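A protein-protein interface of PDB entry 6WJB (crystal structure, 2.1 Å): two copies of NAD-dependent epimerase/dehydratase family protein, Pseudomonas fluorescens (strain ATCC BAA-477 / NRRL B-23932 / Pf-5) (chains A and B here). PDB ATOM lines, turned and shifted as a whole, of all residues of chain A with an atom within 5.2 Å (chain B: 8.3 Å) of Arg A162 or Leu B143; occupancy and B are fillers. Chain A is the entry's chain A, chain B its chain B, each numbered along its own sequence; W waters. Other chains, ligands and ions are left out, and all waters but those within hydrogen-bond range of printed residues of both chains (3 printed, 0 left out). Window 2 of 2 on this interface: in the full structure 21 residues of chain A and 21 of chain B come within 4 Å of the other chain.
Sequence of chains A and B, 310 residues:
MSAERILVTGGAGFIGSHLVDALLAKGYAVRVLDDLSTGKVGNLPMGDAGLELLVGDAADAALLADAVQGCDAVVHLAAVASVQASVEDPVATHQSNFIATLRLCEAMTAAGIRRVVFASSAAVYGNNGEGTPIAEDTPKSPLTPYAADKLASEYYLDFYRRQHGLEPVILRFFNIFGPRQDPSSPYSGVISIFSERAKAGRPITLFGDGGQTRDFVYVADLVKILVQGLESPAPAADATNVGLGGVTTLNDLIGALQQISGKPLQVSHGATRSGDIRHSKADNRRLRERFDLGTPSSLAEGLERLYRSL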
ATOM      1  N   TYR A 155       2.749  28.211 -33.484  1.00  0.00           N
ATOM      2  CA  TYR A 155       3.296  28.435 -32.149  1.00  0.00           C
ATOM      3  C   TYR A 155       2.356  29.284 -31.305  1.00  0.00           C
ATOM      4  O   TYR A 155       2.188  29.032 -30.108  1.00  0.00           O
ATOM      5  CB  TYR A 155       4.666  29.101 -32.246  1.00  0.00           C
ATOM      6  CG  TYR A 155       5.745  28.202 -32.813  1.00  0.00           C
ATOM      7  CD1 TYR A 155       5.810  26.857 -32.474  1.00  0.00           C
ATOM      8  CD2 TYR A 155       6.706  28.705 -33.670  1.00  0.00           C
ATOM      9  CE1 TYR A 155       6.810  26.038 -32.986  1.00  0.00           C
ATOM     10  CE2 TYR A 155       7.701  27.901 -34.184  1.00  0.00           C
ATOM     11  CZ  TYR A 155       7.754  26.576 -33.847  1.00  0.00           C
ATOM     12  OH  TYR A 155       8.760  25.788 -34.369  1.00  0.00           O
ATOM     13  N   ASP A 158      -0.520  27.138 -30.230  1.00  0.00           N
ATOM     14  CA  ASP A 158      -0.146  26.289 -29.099  1.00  0.00           C
ATOM     15  C   ASP A 158      -0.102  27.082 -27.793  1.00  0.00           C
ATOM     16  O   ASP A 158      -0.453  26.558 -26.725  1.00  0.00           O
ATOM     17  CB  ASP A 158       1.210  25.620 -29.342  1.00  0.00           C
ATOM     18  CG  ASP A 158       1.566  24.639 -28.230  1.00  0.00           C
ATOM     19  OD1 ASP A 158       0.885  23.599 -28.142  1.00  0.00           O
ATOM     20  OD2 ASP A 158       2.482  24.924 -27.418  1.00  0.00           O
ATOM     21  N   PHE A 159       0.353  28.335 -27.846  1.00  0.00           N
ATOM     22  CA  PHE A 159       0.392  29.136 -26.626  1.00  0.00           C
ATOM     23  C   PHE A 159      -1.014  29.411 -26.106  1.00  0.00           C
ATOM     24  O   PHE A 159      -1.261  29.345 -24.897  1.00  0.00           O
ATOM     25  CB  PHE A 159       1.149  30.446 -26.871  1.00  0.00           C
ATOM     26  CG  PHE A 159       0.848  31.517 -25.857  1.00  0.00           C
ATOM     27  CD1 PHE A 159       1.411  31.471 -24.592  1.00  0.00           C
ATOM     28  CD2 PHE A 159      -0.011  32.559 -26.169  1.00  0.00           C
ATOM     29  CE1 PHE A 159       1.125  32.453 -23.646  1.00  0.00           C
ATOM     30  CE2 PHE A 159      -0.305  33.543 -25.233  1.00  0.00           C
ATOM     31  CZ  PHE A 159       0.266  33.490 -23.971  1.00  0.00           C
ATOM     32  N   TYR A 160      -1.953  29.716 -26.998  1.00  0.00           N
ATOM     33  CA  TYR A 160      -3.327  29.944 -26.561  1.00  0.00           C
ATOM     34  C   TYR A 160      -3.968  28.662 -26.033  1.00  0.00           C
ATOM     35  O   TYR A 160      -4.807  28.717 -25.120  1.00  0.00           O
ATOM     36  CB  TYR A 160      -4.138  30.544 -27.712  1.00  0.00           C
ATOM     37  CG  TYR A 160      -3.999  32.052 -27.796  1.00  0.00           C
ATOM     38  CD1 TYR A 160      -2.922  32.637 -28.453  1.00  0.00           C
ATOM     39  CD2 TYR A 160      -4.934  32.891 -27.201  1.00  0.00           C
ATOM     40  CE1 TYR A 160      -2.791  34.014 -28.527  1.00  0.00           C
ATOM     41  CE2 TYR A 160      -4.809  34.275 -27.266  1.00  0.00           C
ATOM     42  CZ  TYR A 160      -3.731  34.827 -27.924  1.00  0.00           C
ATOM     43  OH  TYR A 160      -3.607  36.197 -27.993  1.00  0.00           O
ATOM     44  N   ARG A 161      -3.581  27.502 -26.571  1.00  0.00           N
ATOM     45  CA  ARG A 161      -4.064  26.240 -26.013  1.00  0.00           C
ATOM     46  C   ARG A 161      -3.628  26.091 -24.561  1.00  0.00           C
ATOM     47  O   ARG A 161      -4.450  25.826 -23.676  1.00  0.00           O
ATOM     48  CB  ARG A 161      -3.554  25.057 -26.839  1.00  0.00           C
ATOM     49  CG  ARG A 161      -3.834  23.700 -26.179  1.00  0.00           C
ATOM     50  CD  ARG A 161      -3.213  22.529 -26.960  1.00  0.00           C
ATOM     51  NE  ARG A 161      -1.745  22.532 -26.957  1.00  0.00           N
ATOM     52  CZ  ARG A 161      -0.988  22.044 -25.974  1.00  0.00           C
ATOM     53  NH1 ARG A 161      -1.555  21.517 -24.897  1.00  0.00           N
ATOM     54  NH2 ARG A 161       0.341  22.078 -26.067  1.00  0.00           N
ATOM     55  N   ARG A 162      -2.336  26.282 -24.298  1.00  0.00           N
ATOM     56  CA  ARG A 162      -1.815  26.061 -22.956  1.00  0.00           C
ATOM     57  C   ARG A 162      -2.262  27.158 -21.995  1.00  0.00           C
ATOM     58  O   ARG A 162      -2.620  26.875 -20.847  1.00  0.00           O
ATOM     59  CB  ARG A 162      -0.293  25.967 -23.007  1.00  0.00           C
ATOM     60  CG  ARG A 162       0.205  24.618 -23.461  1.00  0.00           C
ATOM     61  CD  ARG A 162       1.720  24.583 -23.590  1.00  0.00           C
ATOM     62  NE  ARG A 162       2.177  25.360 -24.738  1.00  0.00           N
ATOM     63  CZ  ARG A 162       2.775  26.543 -24.645  1.00  0.00           C
ATOM     64  NH1 ARG A 162       3.154  27.176 -25.744  1.00  0.00           N
ATOM     65  NH2 ARG A 162       3.015  27.077 -23.454  1.00  0.00           N
ATOM     66  N   GLN A 163      -2.267  28.411 -22.455  1.00  0.00           N
ATOM     67  CA  GLN A 163      -2.548  29.557 -21.595  1.00  0.00           C
ATOM     68  C   GLN A 163      -4.035  29.880 -21.472  1.00  0.00           C
ATOM     69  O   GLN A 163      -4.454  30.414 -20.442  1.00  0.00           O
ATOM     70  CB  GLN A 163      -1.810  30.795 -22.119  1.00  0.00           C
ATOM     71  CG  GLN A 163      -1.846  32.009 -21.188  1.00  0.00           C
ATOM     72  CD  GLN A 163      -0.997  31.813 -19.943  1.00  0.00           C
ATOM     73  OE1 GLN A 163       0.059  31.188 -19.988  1.00  0.00           O
ATOM     74  NE2 GLN A 163      -1.464  32.337 -18.826  1.00  0.00           N
ATOM     75  N   HIS A 164      -4.847  29.577 -22.490  1.00  0.00           N
ATOM     76  CA  HIS A 164      -6.236  30.017 -22.489  1.00  0.00           C
ATOM     77  C   HIS A 164      -7.231  28.931 -22.900  1.00  0.00           C
ATOM     78  O   HIS A 164      -8.395  29.255 -23.160  1.00  0.00           O
ATOM     79  CB  HIS A 164      -6.406  31.241 -23.407  1.00  0.00           C
ATOM     80  CG  HIS A 164      -5.539  32.407 -23.036  1.00  0.00           C
ATOM     81  ND1 HIS A 164      -5.710  33.124 -21.869  1.00  0.00           N
ATOM     82  CD2 HIS A 164      -4.499  32.986 -23.682  1.00  0.00           C
ATOM     83  CE1 HIS A 164      -4.809  34.089 -21.810  1.00  0.00           C
ATOM     84  NE2 HIS A 164      -4.060  34.026 -22.898  1.00  0.00           N
ATOM     85  N   GLY A 165      -6.827  27.663 -22.979  1.00  0.00           N
ATOM     86  CA  GLY A 165      -7.785  26.590 -23.207  1.00  0.00           C
ATOM     87  C   GLY A 165      -8.315  26.461 -24.621  1.00  0.00           C
ATOM     88  O   GLY A 165      -9.320  25.767 -24.836  1.00  0.00           O
ATOM     89  N   VAL B  83       9.470  38.436 -20.821  1.00  0.00           N
ATOM     90  CA  VAL B  83       8.670  37.358 -21.401  1.00  0.00           C
ATOM     91  C   VAL B  83       7.247  37.400 -20.858  1.00  0.00           C
ATOM     92  O   VAL B  83       6.276  37.199 -21.598  1.00  0.00           O
ATOM     93  CB  VAL B  83       9.335  35.993 -21.132  1.00  0.00           C
ATOM     94  CG1 VAL B  83       8.424  34.866 -21.577  1.00  0.00           C
ATOM     95  CG2 VAL B  83      10.670  35.903 -21.843  1.00  0.00           C
ATOM     96  N   SER B  86       4.813  39.568 -22.629  1.00  0.00           N
ATOM     97  CA  SER B  86       4.264  39.064 -23.887  1.00  0.00           C
ATOM     98  C   SER B  86       3.116  38.100 -23.641  1.00  0.00           C
ATOM     99  O   SER B  86       2.222  37.979 -24.481  1.00  0.00           O
ATOM    100  CB  SER B  86       5.352  38.377 -24.709  1.00  0.00           C
ATOM    101  OG  SER B  86       5.568  37.065 -24.217  1.00  0.00           O
ATOM    102  N   VAL B  87       3.128  37.405 -22.499  1.00  0.00           N
ATOM    103  CA  VAL B  87       2.016  36.530 -22.145  1.00  0.00           C
ATOM    104  C   VAL B  87       0.788  37.359 -21.802  1.00  0.00           C
ATOM    105  O   VAL B  87      -0.346  36.983 -22.127  1.00  0.00           O
ATOM    106  CB  VAL B  87       2.419  35.608 -20.981  1.00  0.00           C
ATOM    107  CG1 VAL B  87       1.242  34.750 -20.546  1.00  0.00           C
ATOM    108  CG2 VAL B  87       3.609  34.734 -21.381  1.00  0.00           C
ATOM    109  N   ALA B 123      15.255  31.377 -25.224  1.00  0.00           N
ATOM    110  CA  ALA B 123      13.842  31.026 -25.124  1.00  0.00           C
ATOM    111  C   ALA B 123      13.316  30.283 -26.360  1.00  0.00           C
ATOM    112  O   ALA B 123      12.297  29.595 -26.255  1.00  0.00           O
ATOM    113  CB  ALA B 123      13.010  32.289 -24.881  1.00  0.00           C
ATOM    114  N   VAL B 124      13.972  30.394 -27.522  1.00  0.00           N
ATOM    115  CA  VAL B 124      13.441  29.723 -28.715  1.00  0.00           C
ATOM    116  C   VAL B 124      13.484  28.205 -28.569  1.00  0.00           C
ATOM    117  O   VAL B 124      12.721  27.497 -29.241  1.00  0.00           O
ATOM    118  CB  VAL B 124      14.191  30.150 -30.004  1.00  0.00           C
ATOM    119  CG1 VAL B 124      14.125  31.680 -30.225  1.00  0.00           C
ATOM    120  CG2 VAL B 124      15.632  29.669 -29.993  1.00  0.00           C
ATOM    121  N   TYR B 125      14.367  27.682 -27.708  1.00  0.00           N
ATOM    122  CA  TYR B 125      14.448  26.251 -27.466  1.00  0.00           C
ATOM    123  C   TYR B 125      13.348  25.743 -26.550  1.00  0.00           C
ATOM    124  O   TYR B 125      13.107  24.530 -26.512  1.00  0.00           O
ATOM    125  CB  TYR B 125      15.800  25.890 -26.836  1.00  0.00           C
ATOM    126  CG  TYR B 125      16.999  26.334 -27.626  1.00  0.00           C
ATOM    127  CD1 TYR B 125      17.284  25.779 -28.869  1.00  0.00           C
ATOM    128  CD2 TYR B 125      17.855  27.304 -27.126  1.00  0.00           C
ATOM    129  CE1 TYR B 125      18.389  26.176 -29.591  1.00  0.00           C
ATOM    130  CE2 TYR B 125      18.965  27.707 -27.837  1.00  0.00           C
ATOM    131  CZ  TYR B 125      19.229  27.140 -29.066  1.00  0.00           C
ATOM    132  OH  TYR B 125      20.334  27.545 -29.769  1.00  0.00           O
ATOM    133  N   GLY B 126      12.711  26.624 -25.784  1.00  0.00           N
ATOM    134  CA  GLY B 126      11.737  26.154 -24.813  1.00  0.00           C
ATOM    135  C   GLY B 126      12.386  25.168 -23.865  1.00  0.00           C
ATOM    136  O   GLY B 126      13.482  25.411 -23.342  1.00  0.00           O
ATOM    137  N   ASN B 127      11.725  24.023 -23.662  1.00  0.00           N
ATOM    138  CA  ASN B 127      12.214  22.983 -22.762  1.00  0.00           C
ATOM    139  C   ASN B 127      13.087  21.941 -23.447  1.00  0.00           C
ATOM    140  O   ASN B 127      13.569  21.030 -22.767  1.00  0.00           O
ATOM    141  CB  ASN B 127      11.042  22.270 -22.089  1.00  0.00           C
ATOM    142  CG  ASN B 127      10.708  22.855 -20.750  1.00  0.00           C
ATOM    143  OD1 ASN B 127      11.184  22.382 -19.717  1.00  0.00           O
ATOM    144  ND2 ASN B 127       9.886  23.894 -20.749  1.00  0.00           N
ATOM    145  N   ASN B 128      13.289  22.033 -24.762  1.00  0.00           N
ATOM    146  CA  ASN B 128      14.035  20.998 -25.471  1.00  0.00           C
ATOM    147  C   ASN B 128      15.512  21.042 -25.105  1.00  0.00           C
ATOM    148  O   ASN B 128      16.127  22.108 -25.081  1.00  0.00           O
ATOM    149  CB  ASN B 128      13.889  21.167 -26.979  1.00  0.00           C
ATOM    150  CG  ASN B 128      12.522  20.802 -27.466  1.00  0.00           C
ATOM    151  OD1 ASN B 128      11.818  20.005 -26.848  1.00  0.00           O
ATOM    152  ND2 ASN B 128      12.135  21.375 -28.586  1.00  0.00           N
ATOM    153  N   LYS B 140      13.381  23.661 -32.035  1.00  0.00           N
ATOM    154  CA  LYS B 140      12.828  24.828 -31.365  1.00  0.00           C
ATOM    155  C   LYS B 140      11.480  24.498 -30.747  1.00  0.00           C
ATOM    156  O   LYS B 140      10.746  23.632 -31.227  1.00  0.00           O
ATOM    157  CB  LYS B 140      12.687  25.986 -32.348  1.00  0.00           C
ATOM    158  CG  LYS B 140      13.957  26.250 -33.129  1.00  0.00           C
ATOM    159  CD  LYS B 140      15.125  26.492 -32.189  1.00  0.00           C
ATOM    160  CE  LYS B 140      16.430  26.593 -32.959  1.00  0.00           C
ATOM    161  NZ  LYS B 140      16.710  25.314 -33.724  1.00  0.00           N
ATOM    162  N   SER B 141      11.155  25.198 -29.660  1.00  0.00           N
ATOM    163  CA  SER B 141       9.858  25.041 -29.004  1.00  0.00           C
ATOM    164  C   SER B 141       9.519  26.327 -28.259  1.00  0.00           C
ATOM    165  O   SER B 141       9.488  26.353 -27.023  1.00  0.00           O
ATOM    166  CB  SER B 141       9.882  23.842 -28.061  1.00  0.00           C
ATOM    167  OG  SER B 141       8.613  23.623 -27.492  1.00  0.00           O
ATOM    168  N   PRO B 142       9.275  27.418 -28.985  1.00  0.00           N
ATOM    169  CA  PRO B 142       8.953  28.683 -28.309  1.00  0.00           C
ATOM    170  C   PRO B 142       7.599  28.580 -27.623  1.00  0.00           C
ATOM    171  O   PRO B 142       6.609  28.201 -28.248  1.00  0.00           O
ATOM    172  CB  PRO B 142       8.933  29.705 -29.452  1.00  0.00           C
ATOM    173  CG  PRO B 142       8.661  28.880 -30.677  1.00  0.00           C
ATOM    174  CD  PRO B 142       9.325  27.578 -30.451  1.00  0.00           C
ATOM    175  N   LEU B 143       7.561  28.926 -26.327  1.00  0.00           N
ATOM    176  CA  LEU B 143       6.380  28.680 -25.505  1.00  0.00           C
ATOM    177  C   LEU B 143       5.542  29.924 -25.244  1.00  0.00           C
ATOM    178  O   LEU B 143       4.411  29.792 -24.765  1.00  0.00           O
ATOM    179  CB  LEU B 143       6.786  28.050 -24.151  1.00  0.00           C
ATOM    180  CG  LEU B 143       7.493  26.696 -24.236  1.00  0.00           C
ATOM    181  CD1 LEU B 143       8.061  26.304 -22.879  1.00  0.00           C
ATOM    182  CD2 LEU B 143       6.552  25.601 -24.760  1.00  0.00           C
ATOM    183  N   THR B 144       6.059  31.108 -25.544  1.00  0.00           N
ATOM    184  CA  THR B 144       5.404  32.386 -25.312  1.00  0.00           C
ATOM    185  C   THR B 144       5.427  33.202 -26.599  1.00  0.00           C
ATOM    186  O   THR B 144       6.226  32.923 -27.494  1.00  0.00           O
ATOM    187  CB  THR B 144       6.116  33.176 -24.206  1.00  0.00           C
ATOM    188  OG1 THR B 144       7.462  33.444 -24.622  1.00  0.00           O
ATOM    189  CG2 THR B 144       6.125  32.380 -22.875  1.00  0.00           C
ATOM    190  N   PRO B 145       4.574  34.230 -26.707  1.00  0.00           N
ATOM    191  CA  PRO B 145       4.684  35.127 -27.874  1.00  0.00           C
ATOM    192  C   PRO B 145       6.072  35.722 -28.042  1.00  0.00           C
ATOM    193  O   PRO B 145       6.541  35.856 -29.176  1.00  0.00           O
ATOM    194  CB  PRO B 145       3.628  36.209 -27.582  1.00  0.00           C
ATOM    195  CG  PRO B 145       2.570  35.462 -26.784  1.00  0.00           C
ATOM    196  CD  PRO B 145       3.407  34.566 -25.870  1.00  0.00           C
ATOM    197  N   TYR B 146       6.740  36.089 -26.940  1.00  0.00           N
ATOM    198  CA  TYR B 146       8.098  36.621 -27.036  1.00  0.00           C
ATOM    199  C   TYR B 146       9.031  35.633 -27.725  1.00  0.00           C
ATOM    200  O   TYR B 146       9.759  35.991 -28.659  1.00  0.00           O
ATOM    201  CB  TYR B 146       8.619  36.959 -25.639  1.00  0.00           C
ATOM    202  CG  TYR B 146      10.107  37.247 -25.559  1.00  0.00           C
ATOM    203  CD1 TYR B 146      10.593  38.540 -25.745  1.00  0.00           C
ATOM    204  CD2 TYR B 146      11.019  36.240 -25.261  1.00  0.00           C
ATOM    205  CE1 TYR B 146      11.947  38.821 -25.640  1.00  0.00           C
ATOM    206  CE2 TYR B 146      12.381  36.506 -25.154  1.00  0.00           C
ATOM    207  CZ  TYR B 146      12.835  37.805 -25.349  1.00  0.00           C
ATOM    208  OH  TYR B 146      14.175  38.088 -25.255  1.00  0.00           O
ATOM    209  N   ALA B 147       9.039  34.383 -27.261  1.00  0.00           N
ATOM    210  CA  ALA B 147       9.958  33.401 -27.830  1.00  0.00           C
ATOM    211  C   ALA B 147       9.626  33.124 -29.295  1.00  0.00           C
ATOM    212  O   ALA B 147      10.525  32.947 -30.125  1.00  0.00           O
ATOM    213  CB  ALA B 147       9.906  32.107 -27.010  1.00  0.00           C
ATOM    214  N   ALA B 148       8.336  33.083 -29.630  1.00  0.00           N
ATOM    215  CA  ALA B 148       7.952  32.835 -31.014  1.00  0.00           C
ATOM    216  C   ALA B 148       8.326  34.008 -31.911  1.00  0.00           C
ATOM    217  O   ALA B 148       8.665  33.809 -33.086  1.00  0.00           O
ATOM    218  CB  ALA B 148       6.451  32.551 -31.091  1.00  0.00           C
ATOM    219  N   ASP B 149       8.280  35.228 -31.373  1.00  0.00           N
ATOM    220  CA  ASP B 149       8.626  36.410 -32.157  1.00  0.00           C
ATOM    221  C   ASP B 149      10.124  36.501 -32.383  1.00  0.00           C
ATOM    222  O   ASP B 149      10.568  36.974 -33.438  1.00  0.00           O
ATOM    223  CB  ASP B 149       8.133  37.679 -31.454  1.00  0.00           C
ATOM    224  CG  ASP B 149       6.629  37.856 -31.547  1.00  0.00           C
ATOM    225  OD1 ASP B 149       5.959  37.101 -32.296  1.00  0.00           O
ATOM    226  OD2 ASP B 149       6.120  38.756 -30.856  1.00  0.00           O
ATOM    227  N   LEU B 151      12.100  33.878 -32.613  1.00  0.00           N
ATOM    228  CA  LEU B 151      12.370  32.867 -33.635  1.00  0.00           C
ATOM    229  C   LEU B 151      11.878  33.330 -35.010  1.00  0.00           C
ATOM    230  O   LEU B 151      12.594  33.218 -36.008  1.00  0.00           O
ATOM    231  CB  LEU B 151      11.718  31.541 -33.241  1.00  0.00           C
ATOM    232  CG  LEU B 151      11.964  30.354 -34.186  1.00  0.00           C
ATOM    233  CD1 LEU B 151      13.451  30.133 -34.360  1.00  0.00           C
ATOM    234  CD2 LEU B 151      11.302  29.092 -33.631  1.00  0.00           C
ATOM    235  N   SER B 274       5.391  28.953 -12.522  1.00  0.00           N
ATOM    236  CA  SER B 274       4.806  27.947 -13.406  1.00  0.00           C
ATOM    237  C   SER B 274       5.632  27.737 -14.670  1.00  0.00           C
ATOM    238  O   SER B 274       5.717  26.614 -15.181  1.00  0.00           O
ATOM    239  CB  SER B 274       3.373  28.341 -13.772  1.00  0.00           C
ATOM    240  N   GLY B 275       6.231  28.798 -15.202  1.00  0.00           N
ATOM    241  CA  GLY B 275       6.914  28.653 -16.476  1.00  0.00           C
ATOM    242  C   GLY B 275       8.405  28.421 -16.348  1.00  0.00           C
ATOM    243  O   GLY B 275       9.144  28.573 -17.322  1.00  0.00           O
ATOM    244  N   ASP B 276       8.858  28.036 -15.157  1.00  0.00           N
ATOM    245  CA  ASP B 276      10.283  28.023 -14.840  1.00  0.00           C
ATOM    246  C   ASP B 276      10.958  26.773 -15.401  1.00  0.00           C
ATOM    247  O   ASP B 276      10.593  25.649 -15.039  1.00  0.00           O
ATOM    248  CB  ASP B 276      10.474  28.104 -13.326  1.00  0.00           C
ATOM    249  CG  ASP B 276      11.931  28.124 -12.924  1.00  0.00           C
ATOM    250  OD1 ASP B 276      12.326  27.345 -12.027  1.00  0.00           O
ATOM    251  OD2 ASP B 276      12.682  28.917 -13.523  1.00  0.00           O
ATOM    252  N   ILE B 277      11.949  26.963 -16.274  1.00  0.00           N
ATOM    253  CA  ILE B 277      12.777  25.850 -16.728  1.00  0.00           C
ATOM    254  C   ILE B 277      13.850  25.581 -15.679  1.00  0.00           C
ATOM    255  O   ILE B 277      14.481  26.515 -15.163  1.00  0.00           O
ATOM    256  CB  ILE B 277      13.391  26.142 -18.108  1.00  0.00           C
ATOM    257  CG1 ILE B 277      14.239  24.962 -18.576  1.00  0.00           C
ATOM    258  CG2 ILE B 277      14.252  27.393 -18.094  1.00  0.00           C
ATOM    259  CD1 ILE B 277      14.889  25.193 -19.915  1.00  0.00           C
HETATM  260  O   HOH W   1      -2.551  36.143 -23.746  1.00  0.00           O
HETATM  261  O   HOH W   2       3.699  29.684 -22.105  1.00  0.00           O
HETATM  262  O   HOH W   3       4.008  28.344 -28.071  1.00  0.00           O
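The guanidinium group (NH1) of Arg A162 is in hydrogen-bond range of the backbone carbonyl oxygen (O) of Leu B143, 3.1 Å away.
The side-chain carboxylate (OD2) of Asp A158 lies within salt-bridge range of the guanidinium group (NE) of Arg A162 (2.7 Å).
CD2 of Tyr A155 touches CG of Pro B142 (3.6 Å). Tyr A155 touches Leu B151 (CE2 to CD2, 3.8 Å). Phe A159 touches Val B87. Phe A159 touches Leu B143 (CD1 to O, 3.4 Å). Pro B145 touches Phe A159. CG1 of Val B87 touches CD of Gln A163, 3.7 Å away.
Printed residues of chain B within 4 Å of Tyr A155: Pro B142 (3.6 Å) and Leu B151 (3.8 Å). Of the printed residues of chain B, Phe A159 touches Val B87, Leu B143 and Pro B145. Arg A162 touches just one residue of chain B: Leu B143. Printed residues of chain B within 4 Å of Gln A163: Val B87 (3.7 Å). Of the printed residues of chain A, Val B87 touches Phe A159 and Gln A163. Of the printed residues of chain A, Pro B142 touches Tyr A155 (3.6 Å). Leu B143 touches just these residues of chain A: Phe A159 (3.4 Å) and Arg A162 (3.1 Å). The nearest residue of chain B that does not touch Arg A162 is Pro B142 (4.4 Å).
Of the 24 printed residues of chain B, 5 touch a printed residue of chain A. Hydrophobic or aromatic side chains of chain B within 4 Å of the printed part of chain A: Val B87, Pro B142, Leu B143, Pro B145 and Leu B151. Printed residues of chain A that touch a printed residue of chain B: Tyr A155, Phe A159, Arg A162 and Gln A163. Hydrophobic or aromatic side chains of chain A that line the printed part of chain B: Tyr A155 and Phe A159. Among the printed residues, 7 pairs touch across the chains.
No position is printed for both chains.
Water W3 lies within hydrogen-bond range of O of Pro B142 (2.6 Å), NH1 of Arg A162 (2.7 Å) and O of Tyr A155 (2.8 Å). Water W1 bridges a ring nitrogen (NE2) of His A164 and the backbone carbonyl oxygen (O) of Val B87. Water W2 bridges the backbone carbonyl oxygen (O) of Leu B143 (2.8 Å) and the guanidinium group (NH2) of Arg A162 (3.0 Å).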
